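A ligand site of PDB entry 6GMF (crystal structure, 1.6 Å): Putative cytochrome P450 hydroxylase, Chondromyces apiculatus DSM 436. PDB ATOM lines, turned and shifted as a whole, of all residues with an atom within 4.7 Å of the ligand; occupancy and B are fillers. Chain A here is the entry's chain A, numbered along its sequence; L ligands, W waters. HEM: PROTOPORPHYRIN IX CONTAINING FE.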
ATOM      1  N   ASN A  58     -16.283   5.357 -28.686  1.00  0.00           N
ATOM      2  CA  ASN A  58     -15.373   6.185 -29.499  1.00  0.00           C
ATOM      3  C   ASN A  58     -15.836   6.248 -30.982  1.00  0.00           C
ATOM      4  O   ASN A  58     -15.291   7.014 -31.787  1.00  0.00           O
ATOM      5  CB  ASN A  58     -13.924   5.765 -29.393  1.00  0.00           C
ATOM      6  CG  ASN A  58     -13.226   6.546 -28.300  1.00  0.00           C
ATOM      7  OD1 ASN A  58     -13.741   6.634 -27.202  1.00  0.00           O
ATOM      8  ND2 ASN A  58     -12.095   7.181 -28.635  1.00  0.00           N
ATOM      9  N   TRP A  61     -16.267   9.608 -32.866  1.00  0.00           N
ATOM     10  CA  TRP A  61     -15.258  10.310 -33.661  1.00  0.00           C
ATOM     11  C   TRP A  61     -15.687  10.377 -35.122  1.00  0.00           C
ATOM     12  O   TRP A  61     -15.266  11.278 -35.834  1.00  0.00           O
ATOM     13  CB  TRP A  61     -13.883   9.693 -33.530  1.00  0.00           C
ATOM     14  CG  TRP A  61     -13.137  10.210 -32.347  1.00  0.00           C
ATOM     15  CD1 TRP A  61     -13.017   9.605 -31.137  1.00  0.00           C
ATOM     16  CD2 TRP A  61     -12.505  11.504 -32.248  1.00  0.00           C
ATOM     17  NE1 TRP A  61     -12.269  10.403 -30.315  1.00  0.00           N
ATOM     18  CE2 TRP A  61     -11.930  11.566 -30.969  1.00  0.00           C
ATOM     19  CE3 TRP A  61     -12.311  12.557 -33.141  1.00  0.00           C
ATOM     20  CZ2 TRP A  61     -11.219  12.675 -30.544  1.00  0.00           C
ATOM     21  CZ3 TRP A  61     -11.577  13.655 -32.732  1.00  0.00           C
ATOM     22  CH2 TRP A  61     -11.022  13.696 -31.436  1.00  0.00           C
ATOM     23  N   ILE A  79      -7.366   3.976 -34.835  1.00  0.00           N
ATOM     24  CA  ILE A  79      -7.426   3.441 -33.506  1.00  0.00           C
ATOM     25  C   ILE A  79      -8.346   4.283 -32.594  1.00  0.00           C
ATOM     26  O   ILE A  79      -9.023   3.698 -31.766  1.00  0.00           O
ATOM     27  CB  ILE A  79      -6.022   3.250 -32.903  1.00  0.00           C
ATOM     28  CG1 ILE A  79      -6.055   2.446 -31.619  1.00  0.00           C
ATOM     29  CG2 ILE A  79      -5.325   4.570 -32.744  1.00  0.00           C
ATOM     30  CD1 ILE A  79      -4.718   2.307 -30.960  1.00  0.00           C
ATOM     31  N   VAL A  80      -8.503   5.600 -32.834  1.00  0.00           N
ATOM     32  CA  VAL A  80      -9.241   6.418 -31.923  1.00  0.00           C
ATOM     33  C   VAL A  80     -10.744   6.193 -32.116  1.00  0.00           C
ATOM     34  O   VAL A  80     -11.543   6.611 -31.294  1.00  0.00           O
ATOM     35  CB  VAL A  80      -8.865   7.906 -32.079  1.00  0.00           C
ATOM     36  CG1 VAL A  80      -9.518   8.540 -33.279  1.00  0.00           C
ATOM     37  CG2 VAL A  80      -9.187   8.704 -30.825  1.00  0.00           C
ATOM     38  N   HIS A  87     -10.176  -2.583 -29.750  1.00  0.00           N
ATOM     39  CA  HIS A  87      -9.273  -1.492 -29.381  1.00  0.00           C
ATOM     40  C   HIS A  87      -8.023  -1.983 -28.646  1.00  0.00           C
ATOM     41  O   HIS A  87      -6.927  -1.568 -28.956  1.00  0.00           O
ATOM     42  CB  HIS A  87     -10.026  -0.461 -28.527  1.00  0.00           C
ATOM     43  CG  HIS A  87      -9.112   0.604 -28.039  1.00  0.00           C
ATOM     44  ND1 HIS A  87      -8.598   0.590 -26.741  1.00  0.00           N
ATOM     45  CD2 HIS A  87      -8.527   1.622 -28.695  1.00  0.00           C
ATOM     46  CE1 HIS A  87      -7.732   1.575 -26.632  1.00  0.00           C
ATOM     47  NE2 HIS A  87      -7.675   2.249 -27.796  1.00  0.00           N
ATOM     48  N   ARG A  91      -4.266  -1.549 -29.818  1.00  0.00           N
ATOM     49  CA  ARG A  91      -3.402  -0.654 -29.085  1.00  0.00           C
ATOM     50  C   ARG A  91      -2.123  -1.365 -28.595  1.00  0.00           C
ATOM     51  O   ARG A  91      -1.025  -0.817 -28.616  1.00  0.00           O
ATOM     52  CB  ARG A  91      -4.164   0.003 -27.935  1.00  0.00           C
ATOM     53  CG  ARG A  91      -3.285   0.968 -27.165  1.00  0.00           C
ATOM     54  CD  ARG A  91      -4.082   1.978 -26.407  1.00  0.00           C
ATOM     55  NE  ARG A  91      -3.184   2.707 -25.526  1.00  0.00           N
ATOM     56  CZ  ARG A  91      -3.296   4.011 -25.268  1.00  0.00           C
ATOM     57  NH1 ARG A  91      -4.173   4.742 -25.945  1.00  0.00           N
ATOM     58  NH2 ARG A  91      -2.488   4.569 -24.399  1.00  0.00           N
ATOM     59  N   PHE A  98       5.425   2.106 -31.549  1.00  0.00           N
ATOM     60  CA  PHE A  98       5.432   3.447 -30.961  1.00  0.00           C
ATOM     61  C   PHE A  98       5.515   3.290 -29.443  1.00  0.00           C
ATOM     62  O   PHE A  98       4.533   3.131 -28.742  1.00  0.00           O
ATOM     63  CB  PHE A  98       4.204   4.267 -31.401  1.00  0.00           C
ATOM     64  CG  PHE A  98       4.299   5.753 -31.132  1.00  0.00           C
ATOM     65  CD1 PHE A  98       4.086   6.279 -29.864  1.00  0.00           C
ATOM     66  CD2 PHE A  98       4.675   6.619 -32.142  1.00  0.00           C
ATOM     67  CE1 PHE A  98       4.216   7.629 -29.605  1.00  0.00           C
ATOM     68  CE2 PHE A  98       4.784   7.985 -31.889  1.00  0.00           C
ATOM     69  CZ  PHE A  98       4.521   8.490 -30.634  1.00  0.00           C
ATOM     70  N   ILE A 142       7.835  13.615 -36.870  1.00  0.00           N
ATOM     71  CA  ILE A 142       7.040  12.426 -37.241  1.00  0.00           C
ATOM     72  C   ILE A 142       7.489  11.870 -38.593  1.00  0.00           C
ATOM     73  O   ILE A 142       7.500  10.633 -38.760  1.00  0.00           O
ATOM     74  CB  ILE A 142       5.514  12.609 -37.121  1.00  0.00           C
ATOM     75  CG1 ILE A 142       4.801  11.296 -36.845  1.00  0.00           C
ATOM     76  CG2 ILE A 142       4.933  13.303 -38.353  1.00  0.00           C
ATOM     77  CD1 ILE A 142       5.157  10.670 -35.495  1.00  0.00           C
ATOM     78  N   PHE A 226      -2.488   3.519 -38.883  1.00  0.00           N
ATOM     79  CA  PHE A 226      -1.830   4.030 -37.691  1.00  0.00           C
ATOM     80  C   PHE A 226      -0.809   5.132 -38.058  1.00  0.00           C
ATOM     81  O   PHE A 226      -0.727   6.173 -37.378  1.00  0.00           O
ATOM     82  CB  PHE A 226      -1.246   2.934 -36.818  1.00  0.00           C
ATOM     83  CG  PHE A 226      -0.662   3.455 -35.530  1.00  0.00           C
ATOM     84  CD1 PHE A 226      -1.493   3.941 -34.502  1.00  0.00           C
ATOM     85  CD2 PHE A 226       0.696   3.500 -35.335  1.00  0.00           C
ATOM     86  CE1 PHE A 226      -0.951   4.424 -33.328  1.00  0.00           C
ATOM     87  CE2 PHE A 226       1.233   3.980 -34.153  1.00  0.00           C
ATOM     88  CZ  PHE A 226       0.403   4.442 -33.159  1.00  0.00           C
ATOM     89  N   THR A 229      -2.811   8.101 -38.661  1.00  0.00           N
ATOM     90  CA  THR A 229      -3.300   8.614 -37.350  1.00  0.00           C
ATOM     91  C   THR A 229      -2.216   9.461 -36.692  1.00  0.00           C
ATOM     92  O   THR A 229      -2.531  10.476 -36.057  1.00  0.00           O
ATOM     93  CB  THR A 229      -3.800   7.491 -36.430  1.00  0.00           C
ATOM     94  OG1 THR A 229      -4.978   6.985 -37.064  1.00  0.00           O
ATOM     95  CG2 THR A 229      -4.137   7.949 -35.029  1.00  0.00           C
ATOM     96  N   LEU A 230      -0.955   9.046 -36.779  1.00  0.00           N
ATOM     97  CA  LEU A 230       0.117   9.766 -36.095  1.00  0.00           C
ATOM     98  C   LEU A 230       0.214  11.205 -36.629  1.00  0.00           C
ATOM     99  O   LEU A 230       0.463  12.137 -35.834  1.00  0.00           O
ATOM    100  CB  LEU A 230       1.446   9.029 -36.225  1.00  0.00           C
ATOM    101  CG  LEU A 230       1.527   7.679 -35.502  1.00  0.00           C
ATOM    102  CD1 LEU A 230       2.843   6.987 -35.829  1.00  0.00           C
ATOM    103  CD2 LEU A 230       1.394   7.826 -33.986  1.00  0.00           C
ATOM    104  N   ALA A 233      -3.241  13.006 -35.437  1.00  0.00           N
ATOM    105  CA  ALA A 233      -3.348  13.050 -33.997  1.00  0.00           C
ATOM    106  C   ALA A 233      -2.255  13.947 -33.400  1.00  0.00           C
ATOM    107  O   ALA A 233      -2.477  14.565 -32.345  1.00  0.00           O
ATOM    108  CB  ALA A 233      -3.269  11.654 -33.392  1.00  0.00           C
ATOM    109  N   GLY A 234      -1.095  14.001 -34.078  1.00  0.00           N
ATOM    110  CA  GLY A 234       0.140  14.505 -33.461  1.00  0.00           C
ATOM    111  C   GLY A 234       0.556  15.894 -33.904  1.00  0.00           C
ATOM    112  O   GLY A 234       1.236  16.602 -33.182  1.00  0.00           O
ATOM    113  N   THR A 237      -2.020  19.156 -32.831  1.00  0.00           N
ATOM    114  CA  THR A 237      -2.097  19.257 -31.374  1.00  0.00           C
ATOM    115  C   THR A 237      -0.744  19.693 -30.778  1.00  0.00           C
ATOM    116  O   THR A 237      -0.725  20.536 -29.884  1.00  0.00           O
ATOM    117  CB  THR A 237      -2.484  17.920 -30.759  1.00  0.00           C
ATOM    118  OG1 THR A 237      -1.586  16.986 -31.318  1.00  0.00           O
ATOM    119  CG2 THR A 237      -3.947  17.639 -31.025  1.00  0.00           C
ATOM    120  N   THR A 238       0.328  19.117 -31.249  1.00  0.00           N
ATOM    121  CA  THR A 238       1.678  19.482 -30.671  1.00  0.00           C
ATOM    122  C   THR A 238       2.036  20.902 -31.048  1.00  0.00           C
ATOM    123  O   THR A 238       2.557  21.649 -30.233  1.00  0.00           O
ATOM    124  CB  THR A 238       2.764  18.484 -31.060  1.00  0.00           C
ATOM    125  OG1 THR A 238       2.351  17.186 -30.677  1.00  0.00           O
ATOM    126  CG2 THR A 238       4.072  18.804 -30.390  1.00  0.00           C
ATOM    127  N   LEU A 241       0.134  23.075 -28.679  1.00  0.00           N
ATOM    128  CA  LEU A 241       0.773  23.126 -27.330  1.00  0.00           C
ATOM    129  C   LEU A 241       1.904  24.153 -27.308  1.00  0.00           C
ATOM    130  O   LEU A 241       1.938  25.013 -26.423  1.00  0.00           O
ATOM    131  CB  LEU A 241       1.293  21.731 -27.009  1.00  0.00           C
ATOM    132  CG  LEU A 241       2.096  21.670 -25.708  1.00  0.00           C
ATOM    133  CD1 LEU A 241       1.308  22.217 -24.533  1.00  0.00           C
ATOM    134  CD2 LEU A 241       2.530  20.257 -25.456  1.00  0.00           C
ATOM    135  N   LEU A 274      -0.888  22.825 -20.863  1.00  0.00           N
ATOM    136  CA  LEU A 274      -1.788  21.728 -21.159  1.00  0.00           C
ATOM    137  C   LEU A 274      -3.109  21.902 -20.421  1.00  0.00           C
ATOM    138  O   LEU A 274      -4.183  21.711 -21.000  1.00  0.00           O
ATOM    139  CB  LEU A 274      -1.148  20.386 -20.832  1.00  0.00           C
ATOM    140  CG  LEU A 274      -0.151  19.910 -21.882  1.00  0.00           C
ATOM    141  CD1 LEU A 274       0.729  18.837 -21.330  1.00  0.00           C
ATOM    142  CD2 LEU A 274      -0.818  19.438 -23.161  1.00  0.00           C
ATOM    143  N   PRO A 279      -4.836  21.997 -25.875  1.00  0.00           N
ATOM    144  CA  PRO A 279      -4.879  21.915 -27.332  1.00  0.00           C
ATOM    145  C   PRO A 279      -6.155  21.248 -27.855  1.00  0.00           C
ATOM    146  O   PRO A 279      -6.768  21.813 -28.729  1.00  0.00           O
ATOM    147  CB  PRO A 279      -3.628  21.148 -27.691  1.00  0.00           C
ATOM    148  CG  PRO A 279      -2.646  21.537 -26.630  1.00  0.00           C
ATOM    149  CD  PRO A 279      -3.478  21.669 -25.379  1.00  0.00           C
ATOM    150  N   ALA A 280      -6.439  20.031 -27.352  1.00  0.00           N
ATOM    151  CA  ALA A 280      -7.656  19.377 -27.688  1.00  0.00           C
ATOM    152  C   ALA A 280      -8.733  19.846 -26.700  1.00  0.00           C
ATOM    153  O   ALA A 280      -8.700  19.439 -25.522  1.00  0.00           O
ATOM    154  CB  ALA A 280      -7.471  17.898 -27.669  1.00  0.00           C
ATOM    155  N   ILE A 283     -13.266  16.142 -27.093  1.00  0.00           N
ATOM    156  CA  ILE A 283     -13.148  14.974 -27.894  1.00  0.00           C
ATOM    157  C   ILE A 283     -14.549  14.462 -28.193  1.00  0.00           C
ATOM    158  O   ILE A 283     -15.495  15.148 -27.850  1.00  0.00           O
ATOM    159  CB  ILE A 283     -12.190  13.976 -27.254  1.00  0.00           C
ATOM    160  CG1 ILE A 283     -12.600  13.559 -25.847  1.00  0.00           C
ATOM    161  CG2 ILE A 283     -10.761  14.545 -27.332  1.00  0.00           C
ATOM    162  CD1 ILE A 283     -11.595  12.621 -25.180  1.00  0.00           C
ATOM    163  N   PHE A 284     -14.659  13.299 -28.842  1.00  0.00           N
ATOM    164  CA  PHE A 284     -15.955  12.832 -29.333  1.00  0.00           C
ATOM    165  C   PHE A 284     -16.322  11.469 -28.765  1.00  0.00           C
ATOM    166  O   PHE A 284     -15.466  10.556 -28.677  1.00  0.00           O
ATOM    167  CB  PHE A 284     -15.915  12.704 -30.858  1.00  0.00           C
ATOM    168  CG  PHE A 284     -15.899  14.038 -31.580  1.00  0.00           C
ATOM    169  CD1 PHE A 284     -14.767  14.822 -31.608  1.00  0.00           C
ATOM    170  CD2 PHE A 284     -17.053  14.520 -32.165  1.00  0.00           C
ATOM    171  CE1 PHE A 284     -14.767  16.032 -32.279  1.00  0.00           C
ATOM    172  CE2 PHE A 284     -17.055  15.723 -32.852  1.00  0.00           C
ATOM    173  CZ  PHE A 284     -15.907  16.472 -32.897  1.00  0.00           C
ATOM    174  N   ARG A 285     -17.622  11.328 -28.413  1.00  0.00           N
ATOM    175  CA  ARG A 285     -18.182  10.042 -27.988  1.00  0.00           C
ATOM    176  C   ARG A 285     -19.602   9.905 -28.575  1.00  0.00           C
ATOM    177  O   ARG A 285     -20.150  10.889 -28.995  1.00  0.00           O
ATOM    178  CB  ARG A 285     -18.238   9.920 -26.464  1.00  0.00           C
ATOM    179  CG  ARG A 285     -16.883   9.966 -25.755  1.00  0.00           C
ATOM    180  CD  ARG A 285     -16.103   8.698 -26.003  1.00  0.00           C
ATOM    181  NE  ARG A 285     -14.897   8.652 -25.174  1.00  0.00           N
ATOM    182  CZ  ARG A 285     -13.699   9.052 -25.566  1.00  0.00           C
ATOM    183  NH1 ARG A 285     -13.544   9.754 -26.685  1.00  0.00           N
ATOM    184  NH2 ARG A 285     -12.643   8.688 -24.831  1.00  0.00           N
ATOM    185  N   LEU A 308     -12.701  18.584 -22.432  1.00  0.00           N
ATOM    186  CA  LEU A 308     -11.427  18.490 -21.681  1.00  0.00           C
ATOM    187  C   LEU A 308     -11.012  19.873 -21.145  1.00  0.00           C
ATOM    188  O   LEU A 308     -10.516  19.976 -19.993  1.00  0.00           O
ATOM    189  CB  LEU A 308     -10.339  17.942 -22.597  1.00  0.00           C
ATOM    190  CG  LEU A 308     -10.644  16.595 -23.238  1.00  0.00           C
ATOM    191  CD1 LEU A 308      -9.445  16.177 -24.036  1.00  0.00           C
ATOM    192  CD2 LEU A 308     -11.028  15.554 -22.218  1.00  0.00           C
ATOM    193  N   ALA A 335      -5.896  16.898 -20.477  1.00  0.00           N
ATOM    194  CA  ALA A 335      -5.514  17.353 -21.811  1.00  0.00           C
ATOM    195  C   ALA A 335      -5.207  16.173 -22.740  1.00  0.00           C
ATOM    196  O   ALA A 335      -5.365  16.340 -23.953  1.00  0.00           O
ATOM    197  CB  ALA A 335      -4.377  18.317 -21.787  1.00  0.00           C
ATOM    198  N   PHE A 336      -4.700  15.043 -22.207  1.00  0.00           N
ATOM    199  CA  PHE A 336      -4.351  13.872 -22.997  1.00  0.00           C
ATOM    200  C   PHE A 336      -5.440  12.802 -22.926  1.00  0.00           C
ATOM    201  O   PHE A 336      -5.209  11.664 -23.330  1.00  0.00           O
ATOM    202  CB  PHE A 336      -3.002  13.340 -22.504  1.00  0.00           C
ATOM    203  CG  PHE A 336      -1.815  14.161 -22.926  1.00  0.00           C
ATOM    204  CD1 PHE A 336      -1.588  14.451 -24.246  1.00  0.00           C
ATOM    205  CD2 PHE A 336      -0.908  14.667 -21.996  1.00  0.00           C
ATOM    206  CE1 PHE A 336      -0.497  15.163 -24.682  1.00  0.00           C
ATOM    207  CE2 PHE A 336       0.171  15.404 -22.418  1.00  0.00           C
ATOM    208  CZ  PHE A 336       0.402  15.647 -23.754  1.00  0.00           C
ATOM    209  N   GLY A 337      -6.624  13.153 -22.404  1.00  0.00           N
ATOM    210  CA  GLY A 337      -7.659  12.218 -22.124  1.00  0.00           C
ATOM    211  C   GLY A 337      -7.362  11.408 -20.871  1.00  0.00           C
ATOM    212  O   GLY A 337      -6.688  11.852 -19.955  1.00  0.00           O
ATOM    213  N   ILE A 340      -8.706   4.268 -21.451  1.00  0.00           N
ATOM    214  CA  ILE A 340      -8.186   3.344 -22.483  1.00  0.00           C
ATOM    215  C   ILE A 340      -7.596   4.066 -23.710  1.00  0.00           C
ATOM    216  O   ILE A 340      -6.670   3.529 -24.334  1.00  0.00           O
ATOM    217  CB  ILE A 340      -9.223   2.296 -22.875  1.00  0.00           C
ATOM    218  CG1 ILE A 340     -10.487   2.858 -23.528  1.00  0.00           C
ATOM    219  CG2 ILE A 340      -9.539   1.422 -21.674  1.00  0.00           C
ATOM    220  CD1 ILE A 340     -11.353   1.781 -24.127  1.00  0.00           C
ATOM    221  N   HIS A 341      -8.168   5.215 -24.088  1.00  0.00           N
ATOM    222  CA  HIS A 341      -7.734   5.943 -25.256  1.00  0.00           C
ATOM    223  C   HIS A 341      -6.716   7.032 -24.919  1.00  0.00           C
ATOM    224  O   HIS A 341      -6.322   7.786 -25.805  1.00  0.00           O
ATOM    225  CB  HIS A 341      -8.918   6.564 -26.010  1.00  0.00           C
ATOM    226  CG  HIS A 341      -9.792   5.563 -26.668  1.00  0.00           C
ATOM    227  ND1 HIS A 341      -9.485   5.003 -27.908  1.00  0.00           N
ATOM    228  CD2 HIS A 341     -10.944   5.006 -26.241  1.00  0.00           C
ATOM    229  CE1 HIS A 341     -10.444   4.175 -28.240  1.00  0.00           C
ATOM    230  NE2 HIS A 341     -11.369   4.158 -27.226  1.00  0.00           N
ATOM    231  N   PHE A 342      -6.163   7.028 -23.704  1.00  0.00           N
ATOM    232  CA  PHE A 342      -5.204   8.033 -23.313  1.00  0.00           C
ATOM    233  C   PHE A 342      -4.148   8.193 -24.412  1.00  0.00           C
ATOM    234  O   PHE A 342      -3.532   7.233 -24.838  1.00  0.00           O
ATOM    235  CB  PHE A 342      -4.532   7.622 -21.998  1.00  0.00           C
ATOM    236  CG  PHE A 342      -3.574   8.628 -21.436  1.00  0.00           C
ATOM    237  CD1 PHE A 342      -3.986   9.673 -20.598  1.00  0.00           C
ATOM    238  CD2 PHE A 342      -2.230   8.560 -21.798  1.00  0.00           C
ATOM    239  CE1 PHE A 342      -3.068  10.604 -20.126  1.00  0.00           C
ATOM    240  CE2 PHE A 342      -1.338   9.510 -21.346  1.00  0.00           C
ATOM    241  CZ  PHE A 342      -1.759  10.525 -20.526  1.00  0.00           C
ATOM    242  N   CYS A 343      -3.782   9.436 -24.710  1.00  0.00           N
ATOM    243  CA  CYS A 343      -2.943   9.791 -25.807  1.00  0.00           C
ATOM    244  C   CYS A 343      -1.664   8.929 -25.832  1.00  0.00           C
ATOM    245  O   CYS A 343      -0.801   9.039 -24.905  1.00  0.00           O
ATOM    246  CB  CYS A 343      -2.540  11.254 -25.699  1.00  0.00           C
ATOM    247  SG  CYS A 343      -1.513  11.811 -27.058  1.00  0.00           S
ATOM    248  N   ILE A 344      -1.479   8.163 -26.896  1.00  0.00           N
ATOM    249  CA  ILE A 344      -0.257   7.401 -27.134  1.00  0.00           C
ATOM    250  C   ILE A 344       0.949   8.348 -27.310  1.00  0.00           C
ATOM    251  O   ILE A 344       2.117   8.015 -26.964  1.00  0.00           O
ATOM    252  CB  ILE A 344      -0.469   6.498 -28.350  1.00  0.00           C
ATOM    253  CG1 ILE A 344      -1.412   5.350 -27.968  1.00  0.00           C
ATOM    254  CG2 ILE A 344       0.830   5.962 -28.942  1.00  0.00           C
ATOM    255  CD1 ILE A 344      -1.864   4.502 -29.116  1.00  0.00           C
ATOM    256  N   GLY A 345       0.711   9.527 -27.863  1.00  0.00           N
ATOM    257  CA  GLY A 345       1.739  10.497 -28.120  1.00  0.00           C
ATOM    258  C   GLY A 345       2.128  11.366 -26.951  1.00  0.00           C
ATOM    259  O   GLY A 345       2.947  12.244 -27.159  1.00  0.00           O
ATOM    260  N   LEU A 348       5.797  12.050 -26.416  1.00  0.00           N
ATOM    261  CA  LEU A 348       6.356  12.734 -27.566  1.00  0.00           C
ATOM    262  C   LEU A 348       5.951  14.213 -27.577  1.00  0.00           C
ATOM    263  O   LEU A 348       6.756  15.058 -27.795  1.00  0.00           O
ATOM    264  CB  LEU A 348       5.969  12.026 -28.865  1.00  0.00           C
ATOM    265  CG  LEU A 348       6.586  12.684 -30.102  1.00  0.00           C
ATOM    266  CD1 LEU A 348       8.121  12.824 -29.962  1.00  0.00           C
ATOM    267  CD2 LEU A 348       6.200  11.911 -31.353  1.00  0.00           C
ATOM    268  N   ALA A 349       4.669  14.526 -27.361  1.00  0.00           N
ATOM    269  CA  ALA A 349       4.222  15.904 -27.267  1.00  0.00           C
ATOM    270  C   ALA A 349       4.987  16.641 -26.178  1.00  0.00           C
ATOM    271  O   ALA A 349       5.415  17.784 -26.346  1.00  0.00           O
ATOM    272  CB  ALA A 349       2.743  15.927 -26.965  1.00  0.00           C
HETATM  273  CHA HEM L   1      -5.314  10.203 -28.329  1.00  0.00           C
HETATM  274  CHB HEM L   1      -4.582  14.661 -27.004  1.00  0.00           C
HETATM  275  CHC HEM L   1      -0.321  14.557 -29.280  1.00  0.00           C
HETATM  276  CHD HEM L   1      -1.239  10.213 -30.936  1.00  0.00           C
HETATM  277  C1A HEM L   1      -5.463  11.424 -27.734  1.00  0.00           C
HETATM  278  C2A HEM L   1      -6.553  11.703 -26.855  1.00  0.00           C
HETATM  279  C3A HEM L   1      -6.356  13.006 -26.503  1.00  0.00           C
HETATM  280  C4A HEM L   1      -5.165  13.437 -27.119  1.00  0.00           C
HETATM  281  CMA HEM L   1      -7.231  13.897 -25.655  1.00  0.00           C
HETATM  282  CAA HEM L   1      -7.700  10.829 -26.431  1.00  0.00           C
HETATM  283  CBA HEM L   1      -8.834  10.725 -27.476  1.00  0.00           C
HETATM  284  CGA HEM L   1     -10.038   9.956 -26.981  1.00  0.00           C
HETATM  285  O1A HEM L   1     -10.101   9.571 -25.789  1.00  0.00           O
HETATM  286  O2A HEM L   1     -10.982   9.859 -27.840  1.00  0.00           O
HETATM  287  C1B HEM L   1      -3.345  15.070 -27.517  1.00  0.00           C
HETATM  288  C2B HEM L   1      -2.710  16.339 -27.267  1.00  0.00           C
HETATM  289  C3B HEM L   1      -1.513  16.344 -27.919  1.00  0.00           C
HETATM  290  C4B HEM L   1      -1.400  15.026 -28.551  1.00  0.00           C
HETATM  291  CMB HEM L   1      -3.355  17.394 -26.476  1.00  0.00           C
HETATM  292  CAB HEM L   1      -0.403  17.369 -27.959  1.00  0.00           C
HETATM  293  CBB HEM L   1      -0.329  18.273 -27.032  1.00  0.00           C
HETATM  294  C1C HEM L   1      -0.128  13.375 -29.896  1.00  0.00           C
HETATM  295  C2C HEM L   1       1.034  13.037 -30.670  1.00  0.00           C
HETATM  296  C3C HEM L   1       0.731  11.761 -31.122  1.00  0.00           C
HETATM  297  C4C HEM L   1      -0.564  11.400 -30.697  1.00  0.00           C
HETATM  298  CMC HEM L   1       2.317  13.799 -30.742  1.00  0.00           C
HETATM  299  CAC HEM L   1       1.530  10.841 -31.940  1.00  0.00           C
HETATM  300  CBC HEM L   1       2.631  11.167 -32.578  1.00  0.00           C
HETATM  301  C1D HEM L   1      -2.438   9.887 -30.368  1.00  0.00           C
HETATM  302  C2D HEM L   1      -3.122   8.595 -30.667  1.00  0.00           C
HETATM  303  C3D HEM L   1      -4.258   8.584 -29.922  1.00  0.00           C
HETATM  304  C4D HEM L   1      -4.264   9.854 -29.186  1.00  0.00           C
HETATM  305  CMD HEM L   1      -2.530   7.560 -31.604  1.00  0.00           C
HETATM  306  CAD HEM L   1      -5.277   7.488 -29.881  1.00  0.00           C
HETATM  307  CBD HEM L   1      -5.126   6.481 -28.733  1.00  0.00           C
HETATM  308  CGD HEM L   1      -6.260   5.466 -28.678  1.00  0.00           C
HETATM  309  O1D HEM L   1      -6.026   4.418 -28.050  1.00  0.00           O
HETATM  310  O2D HEM L   1      -7.360   5.719 -29.227  1.00  0.00           O
HETATM  311  NA  HEM L   1      -4.604  12.499 -27.875  1.00  0.00           N
HETATM  312  NB  HEM L   1      -2.513  14.354 -28.257  1.00  0.00           N
HETATM  313  NC  HEM L   1      -1.112  12.409 -29.954  1.00  0.00           N
HETATM  314  ND  HEM L   1      -3.229  10.634 -29.529  1.00  0.00           N
HETATM  315 FE   HEM L   1      -2.834  12.404 -28.811  1.00  0.00          FE
HETATM  316  O   HOH W   1      -9.036   9.340 -23.363  1.00  0.00           O
HETATM  317  O   HOH W   2      -4.007  13.225 -30.543  1.00  0.00           O
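The side-chain sulfur (SG) of Cys 343 is bound to an iron atom (FE) of the ligand (2.3 Å). A ring nitrogen (ND1) of His 341 lies within hydrogen-bond range of an oxygen (O2D) of the ligand (2.6 Å). O1D of the ligand lies within hydrogen-bond range of NE2 of His 87. NH1 of Arg 285 lies within salt-bridge range of O2A of the ligand (2.8 Å). The guanidinium group (NH1) of Arg 91 is in salt-bridge range of an oxygen (O1D) of the ligand (2.8 Å). An oxygen (O2A) of the ligand is in hydrogen-bond range of the indole nitrogen (NE1) of Trp 61. The side-chain amide nitrogen of Asn 58 sits at hydrogen-bond distance from an oxygen (O2A) of the ligand, at 3.0 Å.
The side-chain sulfur (SG) of Cys 343 sits close to the backbone NH (N) of Gly 345. N of Cys 343 sits at hydrogen-bond distance from O of Phe 336, at 3.0 Å. A ring nitrogen (NE2) of His 87 lies within hydrogen-bond range of a ring nitrogen (ND1) of His 341, 3.3 Å away. A ring nitrogen (NE2) of His 341 sits close to the side-chain amide nitrogen (ND2) of Asn 58 (3.4 Å). O of Phe 342 lies within hydrogen-bond range of NH1 of Arg 91. The side-chain amide nitrogen of Asn 58 lies within hydrogen-bond range of the backbone carbonyl oxygen of Val 80 (2.8 Å). O of Gly 234 lies within hydrogen-bond range of OG1 of Thr 238, at 2.8 Å. The side-chain hydroxyl (OG1) of Thr 237 is in hydrogen-bond range of the backbone carbonyl oxygen (O) of Ala 233 (2.8 Å).
The backbone carbonyl oxygen of Ala 233 lies close to a nitrogen (NC) of the ligand, 3.5 Å away. O of Ile 79 touches O2D of the ligand, at 3.6 Å. Val 80 touches the ligand. CZ of Phe 98 touches CBC of the ligand, 3.8 Å away. CD1 of Ile 142 touches CBC of the ligand, 3.9 Å away. Phe 226 touches the ligand (CE1 to CMD, 3.9 Å). Thr 229 touches the ligand (CG2 to CMD, 3.8 Å). CD2 of Leu 230 touches CAC of the ligand, 3.6 Å away. Gly 234 touches the ligand. Thr 237 touches the ligand (CB to C3B, 3.4 Å). Thr 238 touches the ligand (OG1 to CMC, 3.4 Å). Leu 241 touches the ligand (CB to CBB, 3.8 Å). CB of Pro 279 touches CMB of the ligand (3.96 Å). Ile 283 touches the ligand (CD1 to O1A, 3.5 Å). Leu 308 touches the ligand (CD1 to CMA, 3.6 Å). Ala 335 touches the ligand (O to CMB, 3.4 Å). Phe 336 touches the ligand. Gly 337 touches the ligand. O of Ile 340 touches O1D of the ligand, at 3.9 Å. CD1 of Ile 344 touches CBD of the ligand (3.8 Å). Gly 345 touches the ligand (CA to C3C, 3.4 Å). CD2 of Leu 348 touches CBC of the ligand, at 3.8 Å. CB of Ala 349 touches CAB of the ligand (3.6 Å). Hydrophobic or aromatic side chains within 4 Å of the ligand: Trp 61, Ile 79, Val 80, His 87, Phe 98, Ile 142, Phe 226, Leu 230, Ala 233, Leu 241, Pro 279, Ile 283, Leu 308, Phe 336, His 341, Ile 344, Leu 348 and Ala 349. Within 4 Å of the ligand: Asn 58, Trp 61, Ile 79, Val 80, His 87, Arg 91, Phe 98, Ile 142, Phe 226, Thr 229, Leu 230, Ala 233, Gly 234, Thr 237, Thr 238, Leu 241, Pro 279, Ile 283, Arg 285, Leu 308, Ala 335, Phe 336, Gly 337, Ile 340, His 341, Cys 343, Ile 344, Gly 345, Leu 348 and Ala 349. The nearest printed residue that does not touch the ligand is Leu 274 (4.1 Å).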
